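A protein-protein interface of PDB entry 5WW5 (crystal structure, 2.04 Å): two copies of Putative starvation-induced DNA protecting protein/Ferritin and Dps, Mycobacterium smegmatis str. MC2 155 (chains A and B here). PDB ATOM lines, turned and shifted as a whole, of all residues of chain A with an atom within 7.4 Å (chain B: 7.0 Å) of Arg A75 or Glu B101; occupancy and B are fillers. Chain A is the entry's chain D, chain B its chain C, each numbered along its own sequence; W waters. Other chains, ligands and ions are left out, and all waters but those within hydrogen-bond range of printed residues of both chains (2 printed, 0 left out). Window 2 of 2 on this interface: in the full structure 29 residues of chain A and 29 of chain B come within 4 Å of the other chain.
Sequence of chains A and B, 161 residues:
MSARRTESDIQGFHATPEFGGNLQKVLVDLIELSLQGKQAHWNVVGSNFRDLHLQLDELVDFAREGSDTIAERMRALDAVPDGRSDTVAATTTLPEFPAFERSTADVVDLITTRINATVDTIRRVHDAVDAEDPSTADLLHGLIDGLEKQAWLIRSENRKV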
ATOM      1  N   PHE A  13      -4.398 -23.943 -19.512  1.00  0.00           N
ATOM      2  CA  PHE A  13      -2.984 -24.234 -19.336  1.00  0.00           C
ATOM      3  C   PHE A  13      -2.858 -25.283 -18.238  1.00  0.00           C
ATOM      4  O   PHE A  13      -3.431 -25.123 -17.155  1.00  0.00           O
ATOM      5  CB  PHE A  13      -2.224 -22.953 -18.960  1.00  0.00           C
ATOM      6  CG  PHE A  13      -0.718 -23.104 -18.928  1.00  0.00           C
ATOM      7  CD1 PHE A  13       0.053 -22.805 -20.057  1.00  0.00           C
ATOM      8  CD2 PHE A  13      -0.061 -23.511 -17.758  1.00  0.00           C
ATOM      9  CE1 PHE A  13       1.445 -22.929 -20.025  1.00  0.00           C
ATOM     10  CE2 PHE A  13       1.332 -23.630 -17.723  1.00  0.00           C
ATOM     11  CZ  PHE A  13       2.083 -23.342 -18.859  1.00  0.00           C
ATOM     12  N   LEU A  23       5.805 -26.950  -7.035  1.00  0.00           N
ATOM     13  CA  LEU A  23       4.828 -26.268  -6.179  1.00  0.00           C
ATOM     14  C   LEU A  23       4.514 -27.068  -4.918  1.00  0.00           C
ATOM     15  O   LEU A  23       4.339 -26.482  -3.850  1.00  0.00           O
ATOM     16  CB  LEU A  23       3.548 -25.906  -6.953  1.00  0.00           C
ATOM     17  CG  LEU A  23       3.632 -24.794  -8.014  1.00  0.00           C
ATOM     18  CD1 LEU A  23       2.235 -24.383  -8.469  1.00  0.00           C
ATOM     19  CD2 LEU A  23       4.405 -23.570  -7.527  1.00  0.00           C
ATOM     20  N   ASP A  68      -2.471 -21.745   0.969  1.00  0.00           N
ATOM     21  CA  ASP A  68      -3.731 -21.730   0.220  1.00  0.00           C
ATOM     22  C   ASP A  68      -3.533 -21.232  -1.219  1.00  0.00           C
ATOM     23  O   ASP A  68      -4.063 -21.832  -2.150  1.00  0.00           O
ATOM     24  CB  ASP A  68      -4.803 -20.907   0.951  1.00  0.00           C
ATOM     25  CG  ASP A  68      -6.216 -21.200   0.446  1.00  0.00           C
ATOM     26  OD1 ASP A  68      -6.848 -20.279  -0.100  1.00  0.00           O
ATOM     27  OD2 ASP A  68      -6.709 -22.349   0.579  1.00  0.00           O
ATOM     28  N   THR A  69      -2.769 -20.149  -1.380  1.00  0.00           N
ATOM     29  CA  THR A  69      -2.392 -19.605  -2.684  1.00  0.00           C
ATOM     30  C   THR A  69      -1.698 -20.662  -3.550  1.00  0.00           C
ATOM     31  O   THR A  69      -2.099 -20.878  -4.694  1.00  0.00           O
ATOM     32  CB  THR A  69      -1.478 -18.358  -2.538  1.00  0.00           C
ATOM     33  OG1 THR A  69      -2.172 -17.350  -1.797  1.00  0.00           O
ATOM     34  CG2 THR A  69      -1.083 -17.778  -3.902  1.00  0.00           C
ATOM     35  N   ILE A  70      -0.680 -21.325  -2.996  1.00  0.00           N
ATOM     36  CA  ILE A  70       0.082 -22.319  -3.765  1.00  0.00           C
ATOM     37  C   ILE A  70      -0.789 -23.508  -4.148  1.00  0.00           C
ATOM     38  O   ILE A  70      -0.815 -23.894  -5.316  1.00  0.00           O
ATOM     39  CB  ILE A  70       1.401 -22.760  -3.067  1.00  0.00           C
ATOM     40  CG1 ILE A  70       2.376 -21.569  -2.945  1.00  0.00           C
ATOM     41  CG2 ILE A  70       2.060 -23.938  -3.801  1.00  0.00           C
ATOM     42  CD1 ILE A  70       2.854 -20.953  -4.256  1.00  0.00           C
ATOM     43  N   ALA A  71      -1.521 -24.050  -3.177  1.00  0.00           N
ATOM     44  CA  ALA A  71      -2.402 -25.191  -3.419  1.00  0.00           C
ATOM     45  C   ALA A  71      -3.459 -24.893  -4.482  1.00  0.00           C
ATOM     46  O   ALA A  71      -3.685 -25.710  -5.376  1.00  0.00           O
ATOM     47  CB  ALA A  71      -3.051 -25.645  -2.130  1.00  0.00           C
ATOM     48  N   GLU A  72      -4.086 -23.721  -4.399  1.00  0.00           N
ATOM     49  CA  GLU A  72      -5.138 -23.354  -5.346  1.00  0.00           C
ATOM     50  C   GLU A  72      -4.571 -23.041  -6.734  1.00  0.00           C
ATOM     51  O   GLU A  72      -5.228 -23.304  -7.738  1.00  0.00           O
ATOM     52  CB  GLU A  72      -6.037 -22.236  -4.794  1.00  0.00           C
ATOM     53  CG  GLU A  72      -6.860 -22.736  -3.608  1.00  0.00           C
ATOM     54  CD  GLU A  72      -7.944 -21.787  -3.120  1.00  0.00           C
ATOM     55  OE1 GLU A  72      -7.923 -20.577  -3.443  1.00  0.00           O
ATOM     56  OE2 GLU A  72      -8.829 -22.277  -2.375  1.00  0.00           O
ATOM     57  N   ARG A  73      -3.343 -22.523  -6.778  1.00  0.00           N
ATOM     58  CA  ARG A  73      -2.632 -22.330  -8.046  1.00  0.00           C
ATOM     59  C   ARG A  73      -2.353 -23.673  -8.714  1.00  0.00           C
ATOM     60  O   ARG A  73      -2.512 -23.800  -9.925  1.00  0.00           O
ATOM     61  CB  ARG A  73      -1.326 -21.537  -7.865  1.00  0.00           C
ATOM     62  CG  ARG A  73      -0.598 -21.209  -9.172  1.00  0.00           C
ATOM     63  CD  ARG A  73      -1.486 -20.410 -10.110  1.00  0.00           C
ATOM     64  NE  ARG A  73      -0.861 -20.125 -11.402  1.00  0.00           N
ATOM     65  CZ  ARG A  73      -1.537 -19.848 -12.516  1.00  0.00           C
ATOM     66  NH1 ARG A  73      -2.871 -19.842 -12.513  1.00  0.00           N
ATOM     67  NH2 ARG A  73      -0.879 -19.598 -13.646  1.00  0.00           N
ATOM     68  N   MET A  74      -1.954 -24.664  -7.914  1.00  0.00           N
ATOM     69  CA  MET A  74      -1.834 -26.051  -8.383  1.00  0.00           C
ATOM     70  C   MET A  74      -3.161 -26.544  -8.989  1.00  0.00           C
ATOM     71  O   MET A  74      -3.180 -27.049 -10.119  1.00  0.00           O
ATOM     72  CB  MET A  74      -1.364 -26.979  -7.254  1.00  0.00           C
ATOM     73  CG  MET A  74       0.051 -26.713  -6.771  1.00  0.00           C
ATOM     74  SD  MET A  74       0.515 -27.632  -5.287  1.00  0.00           S
ATOM     75  CE  MET A  74       0.901 -29.233  -5.993  1.00  0.00           C
ATOM     76  N   ARG A  75      -4.259 -26.351  -8.254  1.00  0.00           N
ATOM     77  CA  ARG A  75      -5.601 -26.745  -8.723  1.00  0.00           C
ATOM     78  C   ARG A  75      -5.978 -26.078 -10.051  1.00  0.00           C
ATOM     79  O   ARG A  75      -6.431 -26.748 -10.977  1.00  0.00           O
ATOM     80  CB  ARG A  75      -6.666 -26.452  -7.656  1.00  0.00           C
ATOM     81  CG  ARG A  75      -6.504 -27.192  -6.331  1.00  0.00           C
ATOM     82  CD  ARG A  75      -6.502 -28.704  -6.477  1.00  0.00           C
ATOM     83  NE  ARG A  75      -7.750 -29.235  -7.027  1.00  0.00           N
ATOM     84  CZ  ARG A  75      -7.838 -30.036  -8.092  1.00  0.00           C
ATOM     85  NH1 ARG A  75      -6.746 -30.439  -8.747  1.00  0.00           N
ATOM     86  NH2 ARG A  75      -9.036 -30.459  -8.494  1.00  0.00           N
ATOM     87  N   ALA A  76      -5.757 -24.765 -10.138  1.00  0.00           N
ATOM     88  CA  ALA A  76      -5.985 -23.999 -11.361  1.00  0.00           C
ATOM     89  C   ALA A  76      -5.227 -24.587 -12.560  1.00  0.00           C
ATOM     90  O   ALA A  76      -5.769 -24.660 -13.664  1.00  0.00           O
ATOM     91  CB  ALA A  76      -5.618 -22.537 -11.153  1.00  0.00           C
ATOM     92  N   LEU A  77      -3.997 -25.038 -12.319  1.00  0.00           N
ATOM     93  CA  LEU A  77      -3.152 -25.614 -13.362  1.00  0.00           C
ATOM     94  C   LEU A  77      -3.264 -27.140 -13.493  1.00  0.00           C
ATOM     95  O   LEU A  77      -2.407 -27.778 -14.113  1.00  0.00           O
ATOM     96  CB  LEU A  77      -1.689 -25.189 -13.152  1.00  0.00           C
ATOM     97  CG  LEU A  77      -1.397 -23.686 -13.243  1.00  0.00           C
ATOM     98  CD1 LEU A  77       0.059 -23.407 -12.913  1.00  0.00           C
ATOM     99  CD2 LEU A  77      -1.752 -23.096 -14.593  1.00  0.00           C
ATOM    100  N   ASP A  78      -4.318 -27.711 -12.907  1.00  0.00           N
ATOM    101  CA  ASP A  78      -4.645 -29.142 -13.019  1.00  0.00           C
ATOM    102  C   ASP A  78      -3.622 -30.029 -12.282  1.00  0.00           C
ATOM    103  O   ASP A  78      -3.411 -31.184 -12.644  1.00  0.00           O
ATOM    104  CB  ASP A  78      -4.790 -29.541 -14.506  1.00  0.00           C
ATOM    105  CG  ASP A  78      -5.666 -30.763 -14.724  1.00  0.00           C
ATOM    106  OD1 ASP A  78      -6.704 -30.910 -14.050  1.00  0.00           O
ATOM    107  OD2 ASP A  78      -5.315 -31.575 -15.606  1.00  0.00           O
ATOM    108  N   ALA A  79      -2.970 -29.464 -11.266  1.00  0.00           N
ATOM    109  CA  ALA A  79      -2.127 -30.231 -10.355  1.00  0.00           C
ATOM    110  C   ALA A  79      -2.887 -30.491  -9.053  1.00  0.00           C
ATOM    111  O   ALA A  79      -3.926 -29.870  -8.787  1.00  0.00           O
ATOM    112  CB  ALA A  79      -0.807 -29.519 -10.103  1.00  0.00           C
ATOM    113  N   VAL A  80      -2.382 -31.431  -8.260  1.00  0.00           N
ATOM    114  CA  VAL A  80      -3.085 -31.886  -7.063  1.00  0.00           C
ATOM    115  C   VAL A  80      -2.166 -31.751  -5.843  1.00  0.00           C
ATOM    116  O   VAL A  80      -1.170 -32.458  -5.748  1.00  0.00           O
ATOM    117  CB  VAL A  80      -3.637 -33.332  -7.224  1.00  0.00           C
ATOM    118  CG1 VAL A  80      -4.465 -33.719  -6.018  1.00  0.00           C
ATOM    119  CG2 VAL A  80      -4.514 -33.445  -8.465  1.00  0.00           C
ATOM    120  N   PRO A  81      -2.485 -30.815  -4.922  1.00  0.00           N
ATOM    121  CA  PRO A  81      -1.687 -30.654  -3.715  1.00  0.00           C
ATOM    122  C   PRO A  81      -1.907 -31.790  -2.719  1.00  0.00           C
ATOM    123  O   PRO A  81      -2.965 -32.429  -2.721  1.00  0.00           O
ATOM    124  CB  PRO A  81      -2.216 -29.339  -3.132  1.00  0.00           C
ATOM    125  CG  PRO A  81      -3.640 -29.279  -3.574  1.00  0.00           C
ATOM    126  CD  PRO A  81      -3.591 -29.837  -4.973  1.00  0.00           C
ATOM    127  N   GLN B  39      -7.120 -29.965   2.775  1.00  0.00           N
ATOM    128  CA  GLN B  39      -6.936 -30.981   1.727  1.00  0.00           C
ATOM    129  C   GLN B  39      -8.237 -31.172   0.933  1.00  0.00           C
ATOM    130  O   GLN B  39      -8.223 -31.071  -0.290  1.00  0.00           O
ATOM    131  CB  GLN B  39      -6.439 -32.304   2.326  1.00  0.00           C
ATOM    132  CG  GLN B  39      -6.168 -33.427   1.317  1.00  0.00           C
ATOM    133  CD  GLN B  39      -4.852 -33.285   0.566  1.00  0.00           C
ATOM    134  OE1 GLN B  39      -4.074 -32.359   0.803  1.00  0.00           O
ATOM    135  NE2 GLN B  39      -4.605 -34.210  -0.373  1.00  0.00           N
ATOM    136  N   HIS B  41     -10.975 -29.181   0.886  1.00  0.00           N
ATOM    137  CA  HIS B  41     -11.291 -27.864   0.302  1.00  0.00           C
ATOM    138  C   HIS B  41     -10.609 -27.663  -1.063  1.00  0.00           C
ATOM    139  O   HIS B  41     -11.259 -27.228  -2.017  1.00  0.00           O
ATOM    140  CB  HIS B  41     -10.901 -26.778   1.325  1.00  0.00           C
ATOM    141  CG  HIS B  41     -10.837 -25.379   0.792  1.00  0.00           C
ATOM    142  ND1 HIS B  41     -11.956 -24.585   0.644  1.00  0.00           N
ATOM    143  CD2 HIS B  41      -9.778 -24.602   0.459  1.00  0.00           C
ATOM    144  CE1 HIS B  41     -11.593 -23.395   0.200  1.00  0.00           C
ATOM    145  NE2 HIS B  41     -10.276 -23.377   0.088  1.00  0.00           N
ATOM    146  N   TRP B  42      -9.323 -28.010  -1.161  1.00  0.00           N
ATOM    147  CA  TRP B  42      -8.600 -27.889  -2.436  1.00  0.00           C
ATOM    148  C   TRP B  42      -9.002 -28.944  -3.459  1.00  0.00           C
ATOM    149  O   TRP B  42      -9.105 -28.637  -4.640  1.00  0.00           O
ATOM    150  CB  TRP B  42      -7.076 -27.956  -2.242  1.00  0.00           C
ATOM    151  CG  TRP B  42      -6.505 -26.904  -1.316  1.00  0.00           C
ATOM    152  CD1 TRP B  42      -6.845 -25.576  -1.258  1.00  0.00           C
ATOM    153  CD2 TRP B  42      -5.484 -27.100  -0.330  1.00  0.00           C
ATOM    154  NE1 TRP B  42      -6.105 -24.937  -0.290  1.00  0.00           N
ATOM    155  CE2 TRP B  42      -5.269 -25.848   0.303  1.00  0.00           C
ATOM    156  CE3 TRP B  42      -4.731 -28.215   0.086  1.00  0.00           C
ATOM    157  CZ2 TRP B  42      -4.317 -25.673   1.322  1.00  0.00           C
ATOM    158  CZ3 TRP B  42      -3.789 -28.043   1.110  1.00  0.00           C
ATOM    159  CH2 TRP B  42      -3.594 -26.777   1.714  1.00  0.00           C
ATOM    160  N   ASN B  43      -9.200 -30.183  -3.005  1.00  0.00           N
ATOM    161  CA  ASN B  43      -9.283 -31.333  -3.915  1.00  0.00           C
ATOM    162  C   ASN B  43     -10.673 -31.872  -4.247  1.00  0.00           C
ATOM    163  O   ASN B  43     -10.803 -32.758  -5.100  1.00  0.00           O
ATOM    164  CB  ASN B  43      -8.358 -32.453  -3.433  1.00  0.00           C
ATOM    165  CG  ASN B  43      -6.899 -32.102  -3.598  1.00  0.00           C
ATOM    166  OD1 ASN B  43      -6.539 -31.308  -4.476  1.00  0.00           O
ATOM    167  ND2 ASN B  43      -6.046 -32.686  -2.763  1.00  0.00           N
ATOM    168  N   VAL B  44     -11.700 -31.332  -3.590  1.00  0.00           N
ATOM    169  CA  VAL B  44     -13.088 -31.687  -3.896  1.00  0.00           C
ATOM    170  C   VAL B  44     -13.442 -31.245  -5.323  1.00  0.00           C
ATOM    171  O   VAL B  44     -13.068 -30.151  -5.739  1.00  0.00           O
ATOM    172  CB  VAL B  44     -14.080 -31.119  -2.841  1.00  0.00           C
ATOM    173  CG1 VAL B  44     -14.121 -29.588  -2.846  1.00  0.00           C
ATOM    174  CG2 VAL B  44     -15.469 -31.728  -2.994  1.00  0.00           C
ATOM    175  N   VAL B  45     -14.113 -32.121  -6.069  1.00  0.00           N
ATOM    176  CA  VAL B  45     -14.626 -31.809  -7.414  1.00  0.00           C
ATOM    177  C   VAL B  45     -16.023 -32.422  -7.574  1.00  0.00           C
ATOM    178  O   VAL B  45     -16.394 -33.316  -6.813  1.00  0.00           O
ATOM    179  CB  VAL B  45     -13.674 -32.268  -8.581  1.00  0.00           C
ATOM    180  CG1 VAL B  45     -12.298 -31.616  -8.495  1.00  0.00           C
ATOM    181  CG2 VAL B  45     -13.541 -33.788  -8.683  1.00  0.00           C
ATOM    182  N   PHE B  49     -19.716 -28.527  -6.088  1.00  0.00           N
ATOM    183  CA  PHE B  49     -18.340 -28.210  -5.698  1.00  0.00           C
ATOM    184  C   PHE B  49     -18.260 -26.946  -4.829  1.00  0.00           C
ATOM    185  O   PHE B  49     -17.648 -26.971  -3.764  1.00  0.00           O
ATOM    186  CB  PHE B  49     -17.423 -28.043  -6.935  1.00  0.00           C
ATOM    187  CG  PHE B  49     -16.183 -27.233  -6.656  1.00  0.00           C
ATOM    188  CD1 PHE B  49     -15.078 -27.812  -6.026  1.00  0.00           C
ATOM    189  CD2 PHE B  49     -16.123 -25.878  -6.996  1.00  0.00           C
ATOM    190  CE1 PHE B  49     -13.942 -27.058  -5.740  1.00  0.00           C
ATOM    191  CE2 PHE B  49     -14.992 -25.122  -6.715  1.00  0.00           C
ATOM    192  CZ  PHE B  49     -13.897 -25.713  -6.088  1.00  0.00           C
ATOM    193  N   PRO B  98      -7.850 -39.364   2.289  1.00  0.00           N
ATOM    194  CA  PRO B  98      -7.179 -39.825   1.060  1.00  0.00           C
ATOM    195  C   PRO B  98      -6.536 -38.704   0.249  1.00  0.00           C
ATOM    196  O   PRO B  98      -6.955 -37.546   0.341  1.00  0.00           O
ATOM    197  CB  PRO B  98      -8.314 -40.470   0.256  1.00  0.00           C
ATOM    198  CG  PRO B  98      -9.572 -39.864   0.796  1.00  0.00           C
ATOM    199  CD  PRO B  98      -9.303 -39.638   2.253  1.00  0.00           C
ATOM    200  N   ALA B  99      -5.515 -39.059  -0.530  1.00  0.00           N
ATOM    201  CA  ALA B  99      -4.879 -38.145  -1.478  1.00  0.00           C
ATOM    202  C   ALA B  99      -5.780 -37.949  -2.701  1.00  0.00           C
ATOM    203  O   ALA B  99      -6.808 -38.624  -2.829  1.00  0.00           O
ATOM    204  CB  ALA B  99      -3.515 -38.696  -1.898  1.00  0.00           C
ATOM    205  N   PHE B 100      -5.378 -37.034  -3.593  1.00  0.00           N
ATOM    206  CA  PHE B 100      -5.951 -36.876  -4.950  1.00  0.00           C
ATOM    207  C   PHE B 100      -7.336 -36.228  -4.954  1.00  0.00           C
ATOM    208  O   PHE B 100      -7.934 -36.005  -3.894  1.00  0.00           O
ATOM    209  CB  PHE B 100      -5.966 -38.204  -5.754  1.00  0.00           C
ATOM    210  CG  PHE B 100      -4.719 -39.037  -5.595  1.00  0.00           C
ATOM    211  CD1 PHE B 100      -3.500 -38.622  -6.147  1.00  0.00           C
ATOM    212  CD2 PHE B 100      -4.765 -40.252  -4.900  1.00  0.00           C
ATOM    213  CE1 PHE B 100      -2.346 -39.397  -5.993  1.00  0.00           C
ATOM    214  CE2 PHE B 100      -3.614 -41.028  -4.740  1.00  0.00           C
ATOM    215  CZ  PHE B 100      -2.408 -40.600  -5.292  1.00  0.00           C
ATOM    216  N   GLU B 101      -7.833 -35.916  -6.152  1.00  0.00           N
ATOM    217  CA  GLU B 101      -9.193 -35.397  -6.324  1.00  0.00           C
ATOM    218  C   GLU B 101     -10.219 -36.381  -5.777  1.00  0.00           C
ATOM    219  O   GLU B 101     -10.045 -37.595  -5.888  1.00  0.00           O
ATOM    220  CB  GLU B 101      -9.501 -35.117  -7.794  1.00  0.00           C
ATOM    221  CG  GLU B 101      -8.719 -33.968  -8.419  1.00  0.00           C
ATOM    222  CD  GLU B 101      -9.096 -33.735  -9.872  1.00  0.00           C
ATOM    223  OE1 GLU B 101      -9.458 -34.709 -10.574  1.00  0.00           O
ATOM    224  OE2 GLU B 101      -9.045 -32.570 -10.318  1.00  0.00           O
ATOM    225  N   ARG B 102     -11.269 -35.842  -5.168  1.00  0.00           N
ATOM    226  CA  ARG B 102     -12.360 -36.637  -4.625  1.00  0.00           C
ATOM    227  C   ARG B 102     -13.682 -35.968  -4.956  1.00  0.00           C
ATOM    228  O   ARG B 102     -13.785 -34.740  -4.914  1.00  0.00           O
ATOM    229  CB  ARG B 102     -12.220 -36.796  -3.097  1.00  0.00           C
ATOM    230  CG  ARG B 102     -10.969 -37.532  -2.618  1.00  0.00           C
ATOM    231  CD  ARG B 102     -10.994 -39.021  -2.927  1.00  0.00           C
ATOM    232  NE  ARG B 102      -9.634 -39.555  -2.990  1.00  0.00           N
ATOM    233  CZ  ARG B 102      -9.317 -40.831  -3.183  1.00  0.00           C
ATOM    234  NH1 ARG B 102     -10.267 -41.749  -3.328  1.00  0.00           N
ATOM    235  NH2 ARG B 102      -8.040 -41.193  -3.227  1.00  0.00           N
ATOM    236  N   SER B 103     -14.688 -36.779  -5.281  1.00  0.00           N
ATOM    237  CA  SER B 103     -16.028 -36.270  -5.592  1.00  0.00           C
ATOM    238  C   SER B 103     -16.650 -35.576  -4.375  1.00  0.00           C
ATOM    239  O   SER B 103     -16.302 -35.887  -3.225  1.00  0.00           O
ATOM    240  CB  SER B 103     -16.951 -37.391  -6.073  1.00  0.00           C
ATOM    241  OG  SER B 103     -17.364 -38.184  -4.979  1.00  0.00           O
ATOM    242  N   VAL B 107     -16.339 -36.694  -0.449  1.00  0.00           N
ATOM    243  CA  VAL B 107     -15.832 -35.686   0.501  1.00  0.00           C
ATOM    244  C   VAL B 107     -16.821 -35.445   1.658  1.00  0.00           C
ATOM    245  O   VAL B 107     -16.421 -35.430   2.827  1.00  0.00           O
ATOM    246  CB  VAL B 107     -15.413 -34.379  -0.214  1.00  0.00           C
ATOM    247  CG1 VAL B 107     -15.176 -33.243   0.774  1.00  0.00           C
ATOM    248  CG2 VAL B 107     -14.137 -34.619  -0.999  1.00  0.00           C
HETATM  249  O   HOH W   1     -10.870 -28.946  -6.801  1.00  0.00           O
HETATM  250  O   HOH W   2      -3.225 -35.209  -3.072  1.00  0.00           O
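Water W1 lies within hydrogen-bond range of O of Val B44, O of Trp B42 and NH2 of Arg A75. Water W2 lies within hydrogen-bond range of O of Pro A81, N of Phe B100 and NE2 of Gln B39.
NH1 of Arg A75 is in hydrogen-bond range of O of Ala A79, 2.9 Å away. O of Arg B102 is in hydrogen-bond range of N of Val B45 (2.9 Å). O of Asn B43 lies within hydrogen-bond range of N of Arg B102. The side-chain amide nitrogen (NE2) of Gln B39 lies close to the side-chain amide nitrogen (ND2) of Asn B43 (3.2 Å).
No position is printed for both chains.
Of the 16 printed residues of chain A, 6 touch a printed residue of chain B. Printed residues of chain A that touch a printed residue of chain B: Asp A68, Ala A71, Glu A72, Arg A75, Val A80 and Pro A81. Hydrophobic or aromatic side chains of chain A that line the printed part of chain B: Ala A71, Val A80 and Pro A81. Of the 14 printed residues of chain B, 7 touch a printed residue of chain A. Hydrophobic or aromatic side chains of chain B that line the printed part of chain A: His B41, Trp B42 and Val B45. Among the printed residues, 14 pairs touch across the chains. Among the printed residues, Asp or Glu carboxylates within 4 Å of a Lys or Arg side-chain nitrogen of the other chain: Arg A75 with Glu B101 (2.8 Å).
The side-chain amide nitrogen (ND2) of Asn B43 lies within hydrogen-bond range of the backbone carbonyl oxygen (O) of Pro A81. The side-chain carboxylate (OE2) of Glu B101 is in salt-bridge range of the guanidinium group (NH2) of Arg A75 (2.8 Å). NE2 of His B41 sits at hydrogen-bond distance from OE2 of Glu A72 (3.1 Å). The side-chain amide nitrogen of Gln B39 sits at hydrogen-bond distance from the backbone carbonyl oxygen of Pro A81 (3.4 Å). NE of Arg A75 is in hydrogen-bond range of O of Trp B42. NE1 of Trp B42 sits at hydrogen-bond distance from OD2 of Asp A68, at 2.8 Å.
Among the printed residues, pairs that only touch across the chains: Asp A68 with His B41, Ala A71 with Trp B42, Glu A72 with Trp B42, Arg A75 with Asn B43, Arg A75 with Val B45, Val A80 with Asn B43, Val A80 with Phe B100 and Pro A81 with Trp B42.
Arg A75 touches just these residues of chain B: Trp B42 (2.8 Å), Asn B43 (3.3 Å), Val B45 (3.5 Å) and Glu B101 (2.8 Å). Of the printed residues of chain A, Gln B39 touches Pro A81 (3.4 Å). Of the printed residues of chain A, Trp B42 touches Asp A68 (2.8 Å), Ala A71 (3.3 Å), Glu A72 (3.7 Å), Arg A75 (2.8 Å) and Pro A81 (3.9 Å). Printed residues of chain A within 4 Å of Val B45: Arg A75. Of the printed residues of chain A, Phe B100 touches Val A80 (3.6 Å). Of chain A, only Arg A75 comes within 4 Å of Glu B101. The nearest residue of chain B that does not touch Arg A75 is Val B44 (4.9 Å). The nearest residue of chain A that does not touch Glu B101 is Val A80 (4.02 Å). The nearest printed residue of chain A that does not touch Gln B39 is Val A80 (5.7 Å).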
